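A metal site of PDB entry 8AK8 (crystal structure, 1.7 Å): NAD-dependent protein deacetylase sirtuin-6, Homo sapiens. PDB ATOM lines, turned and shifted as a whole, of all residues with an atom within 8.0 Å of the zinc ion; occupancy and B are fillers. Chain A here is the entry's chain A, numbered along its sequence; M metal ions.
The nearest printed residue that does not touch the zinc ion is Lys 137 (4.6 Å).
The backbone NH (N) of Gly 173 sits close to the side-chain sulfur (SG) of Cys 171 (3.6 Å).
The backbone carbonyl oxygen of Cys 160 sits at hydrogen-bond distance from the backbone NH of Arg 172 (3.2 Å).
SG of Cys 135 lies close to N of Lys 137 (3.4 Å).
The backbone carbonyl oxygen (O) of Thr 140 lies within hydrogen-bond range of the backbone NH (N) of Cys 135, at 2.9 Å.
The side-chain hydroxyl (OG1) of Thr 140 sits close to the side-chain sulfur (SG) of Cys 138 (3.2 Å).
The side-chain sulfur (SG) of Cys 160 sits close to the backbone NH (N) of Val 162, 3.7 Å away.
The side-chain hydroxyl of Tyr 142 sits close to the side-chain sulfur of Cys 160 (2.9 Å).
The backbone carbonyl oxygen (O) of Gly 173 lies within hydrogen-bond range of the backbone NH (N) of Cys 160 (2.7 Å).
SG of Cys 138 binds the zinc ion (2.2 Å).
SG of Cys 135 is bound to the zinc ion.
The zinc ion is bound by SG of Cys 160 (2.3 Å).
SG of Cys 171 binds the zinc ion, at 2.4 Å.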
ATOM      1  N   GLU A 134     -25.540 -13.464  -7.450  1.00  0.00           N
ATOM      2  CA  GLU A 134     -25.968 -12.052  -7.619  1.00  0.00           C
ATOM      3  C   GLU A 134     -24.801 -11.119  -7.274  1.00  0.00           C
ATOM      4  O   GLU A 134     -24.141 -11.377  -6.250  1.00  0.00           O
ATOM      5  CB  GLU A 134     -27.182 -11.789  -6.737  1.00  0.00           C
ATOM      6  CG  GLU A 134     -27.640 -10.332  -6.727  1.00  0.00           C
ATOM      7  CD  GLU A 134     -28.912 -10.110  -5.936  1.00  0.00           C
ATOM      8  OE1 GLU A 134     -29.792 -10.984  -5.974  1.00  0.00           O
ATOM      9  OE2 GLU A 134     -29.039  -9.035  -5.314  1.00  0.00           O
ATOM     10  N   CYS A 135     -24.584 -10.100  -8.105  1.00  0.00           N
ATOM     11  CA  CYS A 135     -23.547  -9.065  -7.893  1.00  0.00           C
ATOM     12  C   CYS A 135     -23.999  -8.160  -6.754  1.00  0.00           C
ATOM     13  O   CYS A 135     -25.080  -7.562  -6.871  1.00  0.00           O
ATOM     14  CB  CYS A 135     -23.328  -8.243  -9.162  1.00  0.00           C
ATOM     15  SG  CYS A 135     -22.181  -6.845  -8.960  1.00  0.00           S
ATOM     16  N   ALA A 136     -23.203  -8.044  -5.698  1.00  0.00           N
ATOM     17  CA  ALA A 136     -23.522  -7.156  -4.558  1.00  0.00           C
ATOM     18  C   ALA A 136     -23.633  -5.696  -5.034  1.00  0.00           C
ATOM     19  O   ALA A 136     -24.515  -4.957  -4.538  1.00  0.00           O
ATOM     20  CB  ALA A 136     -22.477  -7.313  -3.491  1.00  0.00           C
ATOM     21  N   LYS A 137     -22.794  -5.287  -5.993  1.00  0.00           N
ATOM     22  CA  LYS A 137     -22.764  -3.886  -6.468  1.00  0.00           C
ATOM     23  C   LYS A 137     -23.989  -3.571  -7.329  1.00  0.00           C
ATOM     24  O   LYS A 137     -24.752  -2.674  -6.927  1.00  0.00           O
ATOM     25  CB  LYS A 137     -21.479  -3.589  -7.258  1.00  0.00           C
ATOM     26  CG  LYS A 137     -20.224  -3.461  -6.416  1.00  0.00           C
ATOM     27  CD  LYS A 137     -19.047  -2.942  -7.212  1.00  0.00           C
ATOM     28  CE  LYS A 137     -17.806  -2.718  -6.376  1.00  0.00           C
ATOM     29  NZ  LYS A 137     -16.705  -2.158  -7.195  1.00  0.00           N
ATOM     30  N   CYS A 138     -24.206  -4.281  -8.447  1.00  0.00           N
ATOM     31  CA  CYS A 138     -25.228  -3.870  -9.443  1.00  0.00           C
ATOM     32  C   CYS A 138     -26.471  -4.767  -9.399  1.00  0.00           C
ATOM     33  O   CYS A 138     -27.382  -4.498 -10.179  1.00  0.00           O
ATOM     34  CB  CYS A 138     -24.663  -3.808 -10.859  1.00  0.00           C
ATOM     35  SG  CYS A 138     -24.273  -5.412 -11.619  1.00  0.00           S
ATOM     36  N   LYS A 139     -26.503  -5.787  -8.535  1.00  0.00           N
ATOM     37  CA  LYS A 139     -27.675  -6.690  -8.317  1.00  0.00           C
ATOM     38  C   LYS A 139     -27.908  -7.580  -9.534  1.00  0.00           C
ATOM     39  O   LYS A 139     -28.929  -8.317  -9.519  1.00  0.00           O
ATOM     40  CB  LYS A 139     -28.929  -5.864  -7.987  1.00  0.00           C
ATOM     41  CG  LYS A 139     -28.763  -4.887  -6.830  1.00  0.00           C
ATOM     42  CD  LYS A 139     -28.335  -5.535  -5.525  1.00  0.00           C
ATOM     43  CE  LYS A 139     -28.182  -4.516  -4.406  1.00  0.00           C
ATOM     44  NZ  LYS A 139     -27.834  -5.176  -3.122  1.00  0.00           N
ATOM     45  N   THR A 140     -27.030  -7.542 -10.542  1.00  0.00           N
ATOM     46  CA  THR A 140     -27.169  -8.379 -11.764  1.00  0.00           C
ATOM     47  C   THR A 140     -27.080  -9.835 -11.309  1.00  0.00           C
ATOM     48  O   THR A 140     -26.134 -10.187 -10.589  1.00  0.00           O
ATOM     49  CB  THR A 140     -26.155  -8.044 -12.864  1.00  0.00           C
ATOM     50  OG1 THR A 140     -26.489  -6.769 -13.426  1.00  0.00           O
ATOM     51  CG2 THR A 140     -26.156  -9.052 -13.997  1.00  0.00           C
ATOM     52  N   GLN A 141     -28.068 -10.641 -11.693  1.00  0.00           N
ATOM     53  CA  GLN A 141     -28.109 -12.086 -11.383  1.00  0.00           C
ATOM     54  C   GLN A 141     -27.483 -12.849 -12.547  1.00  0.00           C
ATOM     55  O   GLN A 141     -27.551 -12.395 -13.720  1.00  0.00           O
ATOM     56  CB  GLN A 141     -29.546 -12.484 -11.049  1.00  0.00           C
ATOM     57  CG  GLN A 141     -29.974 -11.904  -9.713  1.00  0.00           C
ATOM     58  CD  GLN A 141     -31.319 -12.416  -9.258  1.00  0.00           C
ATOM     59  OE1 GLN A 141     -32.167 -12.753 -10.068  1.00  0.00           O
ATOM     60  NE2 GLN A 141     -31.531 -12.488  -7.952  1.00  0.00           N
ATOM     61  N   TYR A 142     -26.840 -13.962 -12.217  1.00  0.00           N
ATOM     62  CA  TYR A 142     -26.281 -14.926 -13.171  1.00  0.00           C
ATOM     63  C   TYR A 142     -26.927 -16.266 -12.865  1.00  0.00           C
ATOM     64  O   TYR A 142     -26.891 -16.719 -11.672  1.00  0.00           O
ATOM     65  CB  TYR A 142     -24.765 -14.945 -13.067  1.00  0.00           C
ATOM     66  CG  TYR A 142     -24.108 -13.622 -13.351  1.00  0.00           C
ATOM     67  CD1 TYR A 142     -24.082 -12.621 -12.385  1.00  0.00           C
ATOM     68  CD2 TYR A 142     -23.497 -13.377 -14.569  1.00  0.00           C
ATOM     69  CE1 TYR A 142     -23.446 -11.405 -12.637  1.00  0.00           C
ATOM     70  CE2 TYR A 142     -22.873 -12.176 -14.844  1.00  0.00           C
ATOM     71  CZ  TYR A 142     -22.859 -11.187 -13.877  1.00  0.00           C
ATOM     72  OH  TYR A 142     -22.224 -10.006 -14.154  1.00  0.00           O
ATOM     73  N   LEU A 159     -16.570 -12.735 -10.114  1.00  0.00           N
ATOM     74  CA  LEU A 159     -16.735 -11.264 -10.247  1.00  0.00           C
ATOM     75  C   LEU A 159     -17.730 -10.972 -11.356  1.00  0.00           C
ATOM     76  O   LEU A 159     -17.841 -11.765 -12.310  1.00  0.00           O
ATOM     77  CB  LEU A 159     -15.385 -10.603 -10.537  1.00  0.00           C
ATOM     78  CG  LEU A 159     -14.314 -10.793  -9.458  1.00  0.00           C
ATOM     79  CD1 LEU A 159     -13.087  -9.937  -9.773  1.00  0.00           C
ATOM     80  CD2 LEU A 159     -14.853 -10.449  -8.078  1.00  0.00           C
ATOM     81  N   CYS A 160     -18.420  -9.844 -11.219  1.00  0.00           N
ATOM     82  CA  CYS A 160     -19.457  -9.389 -12.158  1.00  0.00           C
ATOM     83  C   CYS A 160     -18.806  -8.988 -13.487  1.00  0.00           C
ATOM     84  O   CYS A 160     -17.692  -8.421 -13.436  1.00  0.00           O
ATOM     85  CB  CYS A 160     -20.171  -8.194 -11.549  1.00  0.00           C
ATOM     86  SG  CYS A 160     -21.582  -7.724 -12.564  1.00  0.00           S
ATOM     87  N   THR A 161     -19.460  -9.301 -14.604  1.00  0.00           N
ATOM     88  CA  THR A 161     -18.940  -9.159 -15.989  1.00  0.00           C
ATOM     89  C   THR A 161     -19.697  -8.077 -16.753  1.00  0.00           C
ATOM     90  O   THR A 161     -19.420  -7.904 -17.954  1.00  0.00           O
ATOM     91  CB  THR A 161     -19.012 -10.512 -16.733  1.00  0.00           C
ATOM     92  OG1 THR A 161     -20.388 -10.890 -16.868  1.00  0.00           O
ATOM     93  CG2 THR A 161     -18.266 -11.612 -16.017  1.00  0.00           C
ATOM     94  N   VAL A 162     -20.639  -7.380 -16.115  1.00  0.00           N
ATOM     95  CA  VAL A 162     -21.492  -6.340 -16.777  1.00  0.00           C
ATOM     96  C   VAL A 162     -20.588  -5.242 -17.364  1.00  0.00           C
ATOM     97  O   VAL A 162     -19.652  -4.839 -16.661  1.00  0.00           O
ATOM     98  CB  VAL A 162     -22.540  -5.776 -15.794  1.00  0.00           C
ATOM     99  CG1 VAL A 162     -23.193  -4.506 -16.317  1.00  0.00           C
ATOM    100  CG2 VAL A 162     -23.595  -6.818 -15.463  1.00  0.00           C
ATOM    101  N   ALA A 163     -20.893  -4.793 -18.599  1.00  0.00           N
ATOM    102  CA  ALA A 163     -20.046  -3.906 -19.435  1.00  0.00           C
ATOM    103  C   ALA A 163     -19.455  -2.755 -18.613  1.00  0.00           C
ATOM    104  O   ALA A 163     -20.239  -2.065 -17.933  1.00  0.00           O
ATOM    105  CB  ALA A 163     -20.859  -3.376 -20.599  1.00  0.00           C
ATOM    106  N   CYS A 171     -17.845  -3.711 -13.917  1.00  0.00           N
ATOM    107  CA  CYS A 171     -18.383  -3.728 -12.530  1.00  0.00           C
ATOM    108  C   CYS A 171     -17.425  -4.465 -11.594  1.00  0.00           C
ATOM    109  O   CYS A 171     -17.139  -3.941 -10.500  1.00  0.00           O
ATOM    110  CB  CYS A 171     -19.752  -4.402 -12.501  1.00  0.00           C
ATOM    111  SG  CYS A 171     -20.484  -4.389 -10.846  1.00  0.00           S
ATOM    112  N   ARG A 172     -16.976  -5.670 -11.998  1.00  0.00           N
ATOM    113  CA  ARG A 172     -16.058  -6.535 -11.201  1.00  0.00           C
ATOM    114  C   ARG A 172     -16.561  -6.672  -9.759  1.00  0.00           C
ATOM    115  O   ARG A 172     -15.773  -7.071  -8.877  1.00  0.00           O
ATOM    116  CB  ARG A 172     -14.616  -5.993 -11.255  1.00  0.00           C
ATOM    117  CG  ARG A 172     -14.091  -5.769 -12.666  1.00  0.00           C
ATOM    118  CD  ARG A 172     -12.612  -6.087 -12.858  1.00  0.00           C
ATOM    119  NE  ARG A 172     -11.824  -5.956 -11.623  1.00  0.00           N
ATOM    120  CZ  ARG A 172     -11.130  -6.934 -11.041  1.00  0.00           C
ATOM    121  NH1 ARG A 172     -11.088  -8.153 -11.571  1.00  0.00           N
ATOM    122  NH2 ARG A 172     -10.482  -6.697  -9.919  1.00  0.00           N
ATOM    123  N   GLY A 173     -17.857  -6.428  -9.538  1.00  0.00           N
ATOM    124  CA  GLY A 173     -18.497  -6.620  -8.233  1.00  0.00           C
ATOM    125  C   GLY A 173     -18.427  -8.066  -7.784  1.00  0.00           C
ATOM    126  O   GLY A 173     -18.366  -8.965  -8.645  1.00  0.00           O
ATOM    127  N   GLU A 174     -18.440  -8.279  -6.467  1.00  0.00           N
ATOM    128  CA  GLU A 174     -18.399  -9.604  -5.810  1.00  0.00           C
ATOM    129  C   GLU A 174     -19.708 -10.343  -6.118  1.00  0.00           C
ATOM    130  O   GLU A 174     -20.799  -9.793  -5.762  1.00  0.00           O
ATOM    131  CB  GLU A 174     -18.153  -9.382  -4.318  1.00  0.00           C
ATOM    132  CG  GLU A 174     -17.806 -10.633  -3.527  1.00  0.00           C
ATOM    133  CD  GLU A 174     -17.496 -10.330  -2.067  1.00  0.00           C
ATOM    134  OE1 GLU A 174     -16.333 -10.003  -1.775  1.00  0.00           O
ATOM    135  OE2 GLU A 174     -18.417 -10.423  -1.230  1.00  0.00           O
ATOM    136  N   LEU A 175     -19.639 -11.516  -6.747  1.00  0.00           N
ATOM    137  CA  LEU A 175     -20.822 -12.399  -6.893  1.00  0.00           C
ATOM    138  C   LEU A 175     -21.058 -13.151  -5.582  1.00  0.00           C
ATOM    139  O   LEU A 175     -20.098 -13.624  -4.972  1.00  0.00           O
ATOM    140  CB  LEU A 175     -20.648 -13.359  -8.085  1.00  0.00           C
ATOM    141  CG  LEU A 175     -20.477 -12.676  -9.431  1.00  0.00           C
ATOM    142  CD1 LEU A 175     -20.715 -13.644 -10.574  1.00  0.00           C
ATOM    143  CD2 LEU A 175     -21.379 -11.465  -9.559  1.00  0.00           C
HETATM  144 ZN    ZN M   1     -22.221  -6.036 -11.095  1.00  0.00          ZN
